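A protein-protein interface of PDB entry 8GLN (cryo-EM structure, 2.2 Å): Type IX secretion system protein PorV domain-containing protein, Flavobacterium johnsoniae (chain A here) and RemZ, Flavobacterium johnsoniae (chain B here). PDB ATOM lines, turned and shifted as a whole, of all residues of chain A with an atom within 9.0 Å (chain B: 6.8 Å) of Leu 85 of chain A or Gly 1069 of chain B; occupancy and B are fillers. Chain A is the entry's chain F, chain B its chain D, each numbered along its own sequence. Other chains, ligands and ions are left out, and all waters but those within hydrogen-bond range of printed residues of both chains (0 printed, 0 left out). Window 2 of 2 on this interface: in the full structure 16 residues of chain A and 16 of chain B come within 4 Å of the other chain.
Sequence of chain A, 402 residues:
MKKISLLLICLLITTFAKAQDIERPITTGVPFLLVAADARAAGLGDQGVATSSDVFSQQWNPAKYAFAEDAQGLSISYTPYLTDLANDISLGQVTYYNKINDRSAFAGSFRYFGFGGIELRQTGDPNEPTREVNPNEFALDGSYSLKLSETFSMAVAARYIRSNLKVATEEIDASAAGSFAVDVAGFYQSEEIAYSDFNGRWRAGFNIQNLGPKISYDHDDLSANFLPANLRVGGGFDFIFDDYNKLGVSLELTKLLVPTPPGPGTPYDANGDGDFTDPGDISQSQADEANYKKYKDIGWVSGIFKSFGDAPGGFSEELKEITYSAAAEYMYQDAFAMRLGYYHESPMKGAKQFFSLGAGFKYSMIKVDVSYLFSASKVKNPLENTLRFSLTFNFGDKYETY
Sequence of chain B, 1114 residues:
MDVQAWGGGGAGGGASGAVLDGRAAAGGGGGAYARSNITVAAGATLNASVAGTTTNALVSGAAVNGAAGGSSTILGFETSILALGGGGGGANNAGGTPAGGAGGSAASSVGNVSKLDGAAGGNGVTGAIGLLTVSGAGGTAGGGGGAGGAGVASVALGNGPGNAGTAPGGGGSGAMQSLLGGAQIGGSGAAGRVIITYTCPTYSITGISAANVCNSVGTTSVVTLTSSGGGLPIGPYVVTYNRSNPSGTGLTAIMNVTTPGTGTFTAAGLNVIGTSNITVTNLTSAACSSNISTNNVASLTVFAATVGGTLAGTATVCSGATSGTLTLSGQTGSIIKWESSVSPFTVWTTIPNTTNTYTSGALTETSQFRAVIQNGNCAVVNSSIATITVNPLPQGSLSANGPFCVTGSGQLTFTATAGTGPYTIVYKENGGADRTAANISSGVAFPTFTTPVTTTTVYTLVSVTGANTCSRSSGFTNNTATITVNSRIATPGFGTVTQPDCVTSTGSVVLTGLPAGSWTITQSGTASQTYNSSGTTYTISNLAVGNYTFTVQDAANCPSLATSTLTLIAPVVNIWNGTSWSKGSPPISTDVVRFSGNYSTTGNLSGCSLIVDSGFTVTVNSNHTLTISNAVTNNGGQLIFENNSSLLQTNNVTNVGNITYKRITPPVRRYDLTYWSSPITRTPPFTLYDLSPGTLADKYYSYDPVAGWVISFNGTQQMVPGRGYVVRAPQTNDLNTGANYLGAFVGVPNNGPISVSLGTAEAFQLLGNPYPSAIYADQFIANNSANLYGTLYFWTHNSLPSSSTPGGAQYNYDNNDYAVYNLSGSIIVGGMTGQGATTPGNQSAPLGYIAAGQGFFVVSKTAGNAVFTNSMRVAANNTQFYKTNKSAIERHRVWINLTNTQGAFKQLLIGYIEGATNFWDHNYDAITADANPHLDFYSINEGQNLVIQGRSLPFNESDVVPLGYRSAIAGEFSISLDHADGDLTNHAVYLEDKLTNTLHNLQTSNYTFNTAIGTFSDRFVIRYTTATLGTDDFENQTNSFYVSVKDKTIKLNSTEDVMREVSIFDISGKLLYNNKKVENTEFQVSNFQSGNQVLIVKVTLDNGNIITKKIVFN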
ATOM      1  N   TYR A  81      -8.785  13.265 -11.812  1.00  0.00           N
ATOM      2  CA  TYR A  81      -7.730  12.266 -11.731  1.00  0.00           C
ATOM      3  C   TYR A  81      -8.346  10.875 -11.755  1.00  0.00           C
ATOM      4  O   TYR A  81      -9.394  10.645 -11.143  1.00  0.00           O
ATOM      5  CB  TYR A  81      -6.900  12.430 -10.454  1.00  0.00           C
ATOM      6  CG  TYR A  81      -5.857  13.518 -10.522  1.00  0.00           C
ATOM      7  CD1 TYR A  81      -6.209  14.853 -10.394  1.00  0.00           C
ATOM      8  CD2 TYR A  81      -4.516  13.208 -10.703  1.00  0.00           C
ATOM      9  CE1 TYR A  81      -5.257  15.850 -10.450  1.00  0.00           C
ATOM     10  CE2 TYR A  81      -3.557  14.197 -10.761  1.00  0.00           C
ATOM     11  CZ  TYR A  81      -3.932  15.516 -10.634  1.00  0.00           C
ATOM     12  OH  TYR A  81      -2.980  16.505 -10.691  1.00  0.00           O
ATOM     13  N   LEU A  82      -7.683   9.953 -12.454  1.00  0.00           N
ATOM     14  CA  LEU A  82      -8.103   8.553 -12.522  1.00  0.00           C
ATOM     15  C   LEU A  82      -9.572   8.441 -12.922  1.00  0.00           C
ATOM     16  O   LEU A  82     -10.380   7.797 -12.250  1.00  0.00           O
ATOM     17  CB  LEU A  82      -7.839   7.840 -11.196  1.00  0.00           C
ATOM     18  CG  LEU A  82      -6.464   8.064 -10.566  1.00  0.00           C
ATOM     19  CD1 LEU A  82      -6.479   7.676  -9.097  1.00  0.00           C
ATOM     20  CD2 LEU A  82      -5.393   7.289 -11.317  1.00  0.00           C
ATOM     21  N   THR A  83      -9.914   9.090 -14.038  1.00  0.00           N
ATOM     22  CA  THR A  83     -11.312   9.183 -14.452  1.00  0.00           C
ATOM     23  C   THR A  83     -11.911   7.806 -14.707  1.00  0.00           C
ATOM     24  O   THR A  83     -13.056   7.541 -14.325  1.00  0.00           O
ATOM     25  CB  THR A  83     -11.430  10.054 -15.701  1.00  0.00           C
ATOM     26  OG1 THR A  83     -10.590   9.527 -16.735  1.00  0.00           O
ATOM     27  CG2 THR A  83     -11.002  11.475 -15.395  1.00  0.00           C
ATOM     28  N   ASP A  84     -11.153   6.917 -15.350  1.00  0.00           N
ATOM     29  CA  ASP A  84     -11.660   5.577 -15.622  1.00  0.00           C
ATOM     30  C   ASP A  84     -11.883   4.789 -14.338  1.00  0.00           C
ATOM     31  O   ASP A  84     -12.791   3.954 -14.273  1.00  0.00           O
ATOM     32  CB  ASP A  84     -10.698   4.828 -16.542  1.00  0.00           C
ATOM     33  CG  ASP A  84      -9.256   4.947 -16.098  1.00  0.00           C
ATOM     34  OD1 ASP A  84      -8.824   6.075 -15.774  1.00  0.00           O
ATOM     35  OD2 ASP A  84      -8.554   3.915 -16.072  1.00  0.00           O
ATOM     36  N   LEU A  85     -11.074   5.041 -13.311  1.00  0.00           N
ATOM     37  CA  LEU A  85     -11.134   4.254 -12.085  1.00  0.00           C
ATOM     38  C   LEU A  85     -12.193   4.753 -11.111  1.00  0.00           C
ATOM     39  O   LEU A  85     -12.962   3.948 -10.575  1.00  0.00           O
ATOM     40  CB  LEU A  85      -9.766   4.247 -11.401  1.00  0.00           C
ATOM     41  CG  LEU A  85      -8.749   3.258 -11.969  1.00  0.00           C
ATOM     42  CD1 LEU A  85      -7.441   3.340 -11.202  1.00  0.00           C
ATOM     43  CD2 LEU A  85      -9.304   1.844 -11.944  1.00  0.00           C
ATOM     44  N   ALA A  86     -12.255   6.058 -10.864  1.00  0.00           N
ATOM     45  CA  ALA A  86     -13.191   6.592  -9.884  1.00  0.00           C
ATOM     46  C   ALA A  86     -13.488   8.046 -10.218  1.00  0.00           C
ATOM     47  O   ALA A  86     -12.771   8.690 -10.988  1.00  0.00           O
ATOM     48  CB  ALA A  86     -12.645   6.461  -8.460  1.00  0.00           C
ATOM     49  N   ASN A  87     -14.561   8.553  -9.625  1.00  0.00           N
ATOM     50  CA  ASN A  87     -14.963   9.944  -9.749  1.00  0.00           C
ATOM     51  C   ASN A  87     -14.608  10.702  -8.476  1.00  0.00           C
ATOM     52  O   ASN A  87     -14.209  10.121  -7.465  1.00  0.00           O
ATOM     53  CB  ASN A  87     -16.466  10.054 -10.032  1.00  0.00           C
ATOM     54  CG  ASN A  87     -16.775  10.174 -11.510  1.00  0.00           C
ATOM     55  OD1 ASN A  87     -15.871  10.220 -12.344  1.00  0.00           O
ATOM     56  ND2 ASN A  87     -18.059  10.230 -11.841  1.00  0.00           N
ATOM     57  N   ASP A  88     -14.749  12.025  -8.550  1.00  0.00           N
ATOM     58  CA  ASP A  88     -14.555  12.959  -7.444  1.00  0.00           C
ATOM     59  C   ASP A  88     -13.115  13.020  -6.950  1.00  0.00           C
ATOM     60  O   ASP A  88     -12.864  13.577  -5.876  1.00  0.00           O
ATOM     61  CB  ASP A  88     -15.486  12.645  -6.266  1.00  0.00           C
ATOM     62  CG  ASP A  88     -16.932  12.983  -6.563  1.00  0.00           C
ATOM     63  OD1 ASP A  88     -17.249  14.185  -6.684  1.00  0.00           O
ATOM     64  OD2 ASP A  88     -17.754  12.049  -6.677  1.00  0.00           O
ATOM     65  N   ILE A  89     -12.166  12.464  -7.693  1.00  0.00           N
ATOM     66  CA  ILE A  89     -10.745  12.658  -7.433  1.00  0.00           C
ATOM     67  C   ILE A  89     -10.254  13.690  -8.436  1.00  0.00           C
ATOM     68  O   ILE A  89     -10.052  13.377  -9.613  1.00  0.00           O
ATOM     69  CB  ILE A  89      -9.954  11.350  -7.549  1.00  0.00           C
ATOM     70  CG1 ILE A  89     -10.597  10.256  -6.694  1.00  0.00           C
ATOM     71  CG2 ILE A  89      -8.504  11.571  -7.150  1.00  0.00           C
ATOM     72  CD1 ILE A  89      -9.865   8.937  -6.751  1.00  0.00           C
ATOM     73  N   LYS A 380       3.733   6.506 -17.126  1.00  0.00           N
ATOM     74  CA  LYS A 380       2.336   6.883 -17.292  1.00  0.00           C
ATOM     75  C   LYS A 380       2.059   8.232 -16.642  1.00  0.00           C
ATOM     76  O   LYS A 380       2.442   8.476 -15.495  1.00  0.00           O
ATOM     77  CB  LYS A 380       1.426   5.816 -16.690  1.00  0.00           C
ATOM     78  CG  LYS A 380      -0.053   6.071 -16.922  1.00  0.00           C
ATOM     79  CD  LYS A 380      -0.890   4.851 -16.580  1.00  0.00           C
ATOM     80  CE  LYS A 380      -0.646   4.394 -15.151  1.00  0.00           C
ATOM     81  NZ  LYS A 380      -0.684   5.526 -14.186  1.00  0.00           N
ATOM     82  N   ASN A 381       1.392   9.102 -17.379  1.00  0.00           N
ATOM     83  CA  ASN A 381       0.954  10.398 -16.877  1.00  0.00           C
ATOM     84  C   ASN A 381      -0.422  10.251 -16.237  1.00  0.00           C
ATOM     85  O   ASN A 381      -1.352   9.774 -16.896  1.00  0.00           O
ATOM     86  CB  ASN A 381       0.906  11.419 -18.008  1.00  0.00           C
ATOM     87  CG  ASN A 381       0.666  12.840 -17.521  1.00  0.00           C
ATOM     88  OD1 ASN A 381      -0.170  13.089 -16.654  1.00  0.00           O
ATOM     89  ND2 ASN A 381       1.408  13.783 -18.086  1.00  0.00           N
ATOM     90  N   PRO A 382      -0.588  10.633 -14.969  1.00  0.00           N
ATOM     91  CA  PRO A 382      -1.899  10.465 -14.319  1.00  0.00           C
ATOM     92  C   PRO A 382      -3.010  11.272 -14.967  1.00  0.00           C
ATOM     93  O   PRO A 382      -4.187  10.958 -14.754  1.00  0.00           O
ATOM     94  CB  PRO A 382      -1.632  10.928 -12.880  1.00  0.00           C
ATOM     95  CG  PRO A 382      -0.490  11.885 -13.018  1.00  0.00           C
ATOM     96  CD  PRO A 382       0.389  11.264 -14.066  1.00  0.00           C
ATOM     97  N   ASN A 385      -5.807  10.626 -20.801  1.00  0.00           N
ATOM     98  CA  ASN A 385      -7.212  10.302 -21.055  1.00  0.00           C
ATOM     99  C   ASN A 385      -8.150  11.140 -20.192  1.00  0.00           C
ATOM    100  O   ASN A 385      -9.214  10.674 -19.780  1.00  0.00           O
ATOM    101  CB  ASN A 385      -7.487   8.809 -20.842  1.00  0.00           C
ATOM    102  CG  ASN A 385      -6.612   7.926 -21.709  1.00  0.00           C
ATOM    103  OD1 ASN A 385      -6.815   7.827 -22.918  1.00  0.00           O
ATOM    104  ND2 ASN A 385      -5.627   7.283 -21.092  1.00  0.00           N
ATOM    105  N   THR A 386      -7.762  12.382 -19.914  1.00  0.00           N
ATOM    106  CA  THR A 386      -8.513  13.262 -19.029  1.00  0.00           C
ATOM    107  C   THR A 386      -8.800  14.571 -19.748  1.00  0.00           C
ATOM    108  O   THR A 386      -7.898  15.164 -20.348  1.00  0.00           O
ATOM    109  CB  THR A 386      -7.738  13.521 -17.728  1.00  0.00           C
ATOM    110  OG1 THR A 386      -7.933  12.426 -16.826  1.00  0.00           O
ATOM    111  CG2 THR A 386      -8.203  14.809 -17.061  1.00  0.00           C
ATOM    112  N   SER B1063     -11.421  -5.707  -8.325  1.00  0.00           N
ATOM    113  CA  SER B1063     -10.087  -5.174  -8.569  1.00  0.00           C
ATOM    114  C   SER B1063      -9.854  -4.021  -7.607  1.00  0.00           C
ATOM    115  O   SER B1063     -10.645  -3.073  -7.569  1.00  0.00           O
ATOM    116  CB  SER B1063      -9.931  -4.714 -10.020  1.00  0.00           C
ATOM    117  OG  SER B1063     -10.223  -5.766 -10.920  1.00  0.00           O
ATOM    118  N   PHE B1065      -7.408  -0.963  -6.420  1.00  0.00           N
ATOM    119  CA  PHE B1065      -6.395  -0.072  -6.962  1.00  0.00           C
ATOM    120  C   PHE B1065      -5.898   0.882  -5.887  1.00  0.00           C
ATOM    121  O   PHE B1065      -6.692   1.463  -5.141  1.00  0.00           O
ATOM    122  CB  PHE B1065      -6.939   0.742  -8.142  1.00  0.00           C
ATOM    123  CG  PHE B1065      -7.345  -0.088  -9.323  1.00  0.00           C
ATOM    124  CD1 PHE B1065      -8.601  -0.669  -9.381  1.00  0.00           C
ATOM    125  CD2 PHE B1065      -6.475  -0.282 -10.381  1.00  0.00           C
ATOM    126  CE1 PHE B1065      -8.978  -1.429 -10.468  1.00  0.00           C
ATOM    127  CE2 PHE B1065      -6.847  -1.041 -11.472  1.00  0.00           C
ATOM    128  CZ  PHE B1065      -8.099  -1.617 -11.515  1.00  0.00           C
ATOM    129  N   ASP B1066      -4.580   1.034  -5.812  1.00  0.00           N
ATOM    130  CA  ASP B1066      -3.995   2.164  -5.113  1.00  0.00           C
ATOM    131  C   ASP B1066      -4.315   3.415  -5.927  1.00  0.00           C
ATOM    132  O   ASP B1066      -4.619   3.343  -7.120  1.00  0.00           O
ATOM    133  CB  ASP B1066      -2.483   1.918  -4.936  1.00  0.00           C
ATOM    134  CG  ASP B1066      -1.648   3.187  -4.689  1.00  0.00           C
ATOM    135  OD1 ASP B1066      -2.158   4.324  -4.645  1.00  0.00           O
ATOM    136  OD2 ASP B1066      -0.418   3.028  -4.531  1.00  0.00           O
ATOM    137  N   ILE B1067      -4.250   4.580  -5.283  1.00  0.00           N
ATOM    138  CA  ILE B1067      -4.591   5.782  -6.033  1.00  0.00           C
ATOM    139  C   ILE B1067      -3.349   6.229  -6.787  1.00  0.00           C
ATOM    140  O   ILE B1067      -2.732   7.253  -6.472  1.00  0.00           O
ATOM    141  CB  ILE B1067      -5.116   6.885  -5.096  1.00  0.00           C
ATOM    142  CG1 ILE B1067      -4.273   6.927  -3.819  1.00  0.00           C
ATOM    143  CG2 ILE B1067      -6.579   6.655  -4.771  1.00  0.00           C
ATOM    144  CD1 ILE B1067      -4.592   8.075  -2.904  1.00  0.00           C
ATOM    145  N   SER B1068      -2.999   5.458  -7.803  1.00  0.00           N
ATOM    146  CA  SER B1068      -2.058   5.863  -8.836  1.00  0.00           C
ATOM    147  C   SER B1068      -2.406   5.247 -10.180  1.00  0.00           C
ATOM    148  O   SER B1068      -1.656   5.444 -11.139  1.00  0.00           O
ATOM    149  CB  SER B1068      -0.623   5.486  -8.433  1.00  0.00           C
ATOM    150  OG  SER B1068      -0.446   4.082  -8.417  1.00  0.00           O
ATOM    151  N   GLY B1069      -3.511   4.508 -10.283  1.00  0.00           N
ATOM    152  CA  GLY B1069      -3.759   3.627 -11.399  1.00  0.00           C
ATOM    153  C   GLY B1069      -3.156   2.248 -11.253  1.00  0.00           C
ATOM    154  O   GLY B1069      -3.367   1.403 -12.133  1.00  0.00           O
ATOM    155  N   LYS B1070      -2.422   1.988 -10.173  1.00  0.00           N
ATOM    156  CA  LYS B1070      -1.740   0.714  -9.995  1.00  0.00           C
ATOM    157  C   LYS B1070      -2.683  -0.321  -9.393  1.00  0.00           C
ATOM    158  O   LYS B1070      -3.310  -0.077  -8.358  1.00  0.00           O
ATOM    159  CB  LYS B1070      -0.513   0.886  -9.102  1.00  0.00           C
ATOM    160  CG  LYS B1070       0.212  -0.411  -8.790  1.00  0.00           C
ATOM    161  CD  LYS B1070       1.484  -0.159  -7.998  1.00  0.00           C
ATOM    162  CE  LYS B1070       1.989  -1.431  -7.341  1.00  0.00           C
ATOM    163  NZ  LYS B1070       1.692  -2.635  -8.166  1.00  0.00           N
ATOM    164  N   LEU B1071      -2.769  -1.480 -10.039  1.00  0.00           N
ATOM    165  CA  LEU B1071      -3.595  -2.576  -9.551  1.00  0.00           C
ATOM    166  C   LEU B1071      -2.837  -3.356  -8.485  1.00  0.00           C
ATOM    167  O   LEU B1071      -1.764  -3.905  -8.757  1.00  0.00           O
ATOM    168  CB  LEU B1071      -3.996  -3.490 -10.706  1.00  0.00           C
ATOM    169  CG  LEU B1071      -4.804  -4.736 -10.344  1.00  0.00           C
ATOM    170  CD1 LEU B1071      -6.269  -4.388 -10.149  1.00  0.00           C
ATOM    171  CD2 LEU B1071      -4.642  -5.803 -11.412  1.00  0.00           C
ATOM    172  N   ILE B1096      -9.112   2.164  -4.008  1.00  0.00           N
ATOM    173  CA  ILE B1096     -10.319   2.178  -4.826  1.00  0.00           C
ATOM    174  C   ILE B1096     -10.703   0.736  -5.117  1.00  0.00           C
ATOM    175  O   ILE B1096      -9.918  -0.015  -5.710  1.00  0.00           O
ATOM    176  CB  ILE B1096     -10.120   2.966  -6.128  1.00  0.00           C
ATOM    177  CG1 ILE B1096      -9.747   4.415  -5.823  1.00  0.00           C
ATOM    178  CG2 ILE B1096     -11.377   2.908  -6.978  1.00  0.00           C
ATOM    179  CD1 ILE B1096      -9.329   5.198  -7.040  1.00  0.00           C
ATOM    180  N   VAL B1097     -11.904   0.351  -4.706  1.00  0.00           N
ATOM    181  CA  VAL B1097     -12.425  -0.987  -4.944  1.00  0.00           C
ATOM    182  C   VAL B1097     -13.427  -0.907  -6.084  1.00  0.00           C
ATOM    183  O   VAL B1097     -14.419  -0.172  -6.000  1.00  0.00           O
ATOM    184  CB  VAL B1097     -13.071  -1.574  -3.680  1.00  0.00           C
ATOM    185  CG1 VAL B1097     -13.476  -3.017  -3.916  1.00  0.00           C
ATOM    186  CG2 VAL B1097     -12.119  -1.470  -2.502  1.00  0.00           C
ATOM    187  N   LYS B1098     -13.172  -1.656  -7.151  1.00  0.00           N
ATOM    188  CA  LYS B1098     -14.078  -1.746  -8.286  1.00  0.00           C
ATOM    189  C   LYS B1098     -14.576  -3.178  -8.385  1.00  0.00           C
ATOM    190  O   LYS B1098     -13.775  -4.111  -8.500  1.00  0.00           O
ATOM    191  CB  LYS B1098     -13.392  -1.313  -9.582  1.00  0.00           C
ATOM    192  CG  LYS B1098     -12.968   0.144  -9.585  1.00  0.00           C
ATOM    193  CD  LYS B1098     -12.677   0.631 -10.988  1.00  0.00           C
ATOM    194  CE  LYS B1098     -13.961   0.913 -11.743  1.00  0.00           C
ATOM    195  NZ  LYS B1098     -14.682   2.090 -11.197  1.00  0.00           N
ATOM    196  N   THR B1108     -18.090   1.206  -7.817  1.00  0.00           N
ATOM    197  CA  THR B1108     -16.830   1.801  -7.395  1.00  0.00           C
ATOM    198  C   THR B1108     -16.978   2.356  -5.988  1.00  0.00           C
ATOM    199  O   THR B1108     -17.896   3.137  -5.718  1.00  0.00           O
ATOM    200  CB  THR B1108     -16.393   2.911  -8.352  1.00  0.00           C
ATOM    201  OG1 THR B1108     -16.518   2.458  -9.705  1.00  0.00           O
ATOM    202  CG2 THR B1108     -14.952   3.310  -8.080  1.00  0.00           C
ATOM    203  N   LYS B1109     -16.073   1.957  -5.098  1.00  0.00           N
ATOM    204  CA  LYS B1109     -16.062   2.438  -3.725  1.00  0.00           C
ATOM    205  C   LYS B1109     -14.645   2.834  -3.342  1.00  0.00           C
ATOM    206  O   LYS B1109     -13.698   2.082  -3.592  1.00  0.00           O
ATOM    207  CB  LYS B1109     -16.595   1.375  -2.760  1.00  0.00           C
ATOM    208  CG  LYS B1109     -17.123   1.934  -1.450  1.00  0.00           C
ATOM    209  CD  LYS B1109     -18.530   2.498  -1.600  1.00  0.00           C
ATOM    210  CE  LYS B1109     -19.400   1.614  -2.479  1.00  0.00           C
ATOM    211  NZ  LYS B1109     -20.849   1.914  -2.309  1.00  0.00           N
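Among the printed residues, pairs that only touch across the chains: Leu 82 of chain A with Ser 1068 of chain B, Leu 82 of chain A with Gly 1069 of chain B, Leu 85 of chain A with Phe 1065 of chain B, Leu 85 of chain A with Gly 1069 of chain B, Leu 85 of chain A with Thr 1108 of chain B, Ala 86 of chain A with Ile 1096 of chain B, Ala 86 of chain A with Thr 1108 of chain B and Ile 89 of chain A with Ile 1096 of chain B.
The backbone carbonyl oxygen (O) of Leu 85 of chain A sits at hydrogen-bond distance from the side-chain amino group (NZ) of Lys 1098 of chain B (2.6 Å).
The side-chain amino group (NZ) of Lys 380 of chain A sits at hydrogen-bond distance from the backbone carbonyl oxygen (O) of Ser 1068 of chain B (3.2 Å).
Of the 13 printed residues of chain B, 6 touch a printed residue of chain A.
Hydrophobic or aromatic side chains of chain A that line the printed part of chain B: Leu 82, Leu 85, Ala 86 and Ile 89.
Among the printed residues, 10 pairs touch across the chains.
Of the printed residues of chain B, Leu 85 of chain A touches Phe 1065, Gly 1069, Lys 1098 and Thr 1108.
Of chain A, only Leu 82 (3.5 Å) and Leu 85 (3.7 Å) come within 4 Å of Gly 1069 of chain B.
Ser 1068 of chain B touches just these residues of chain A: Leu 82 (3.8 Å) and Lys 380 (3.2 Å).
Of the printed residues of chain B, Lys 380 of chain A touches Ser 1068.
Printed residues of chain B within 4 Å of Ala 86 of chain A: Ile 1096 and Thr 1108.
Of the printed residues of chain B, Leu 82 of chain A touches Ser 1068 (3.8 Å) and Gly 1069 (3.5 Å).
Of the printed residues of chain B, Ile 89 of chain A touches Ile 1096.
Val 1097 of chain B touches none of the printed residues of chain A.
The nearest printed residue of chain A that does not touch Phe 1065 of chain B is Asp 84 of chain A (7.0 Å).
O of Ile 89 of chain A lies within hydrogen-bond range of N of Tyr 81 of chain A, 2.5 Å away.
The backbone carbonyl oxygen of Phe 1065 of chain B sits at hydrogen-bond distance from the backbone NH of Ile 1096 of chain B (2.8 Å).
N of Lys 1070 of chain B lies close to OG of Ser 1068 of chain B (3.4 Å).
N of Ser 1068 of chain B lies close to OD1 of Asp 1066 of chain B (3.5 Å).
The backbone NH (N) of Ser 1063 of chain B is in hydrogen-bond range of the backbone carbonyl oxygen (O) of Lys 1098 of chain B.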
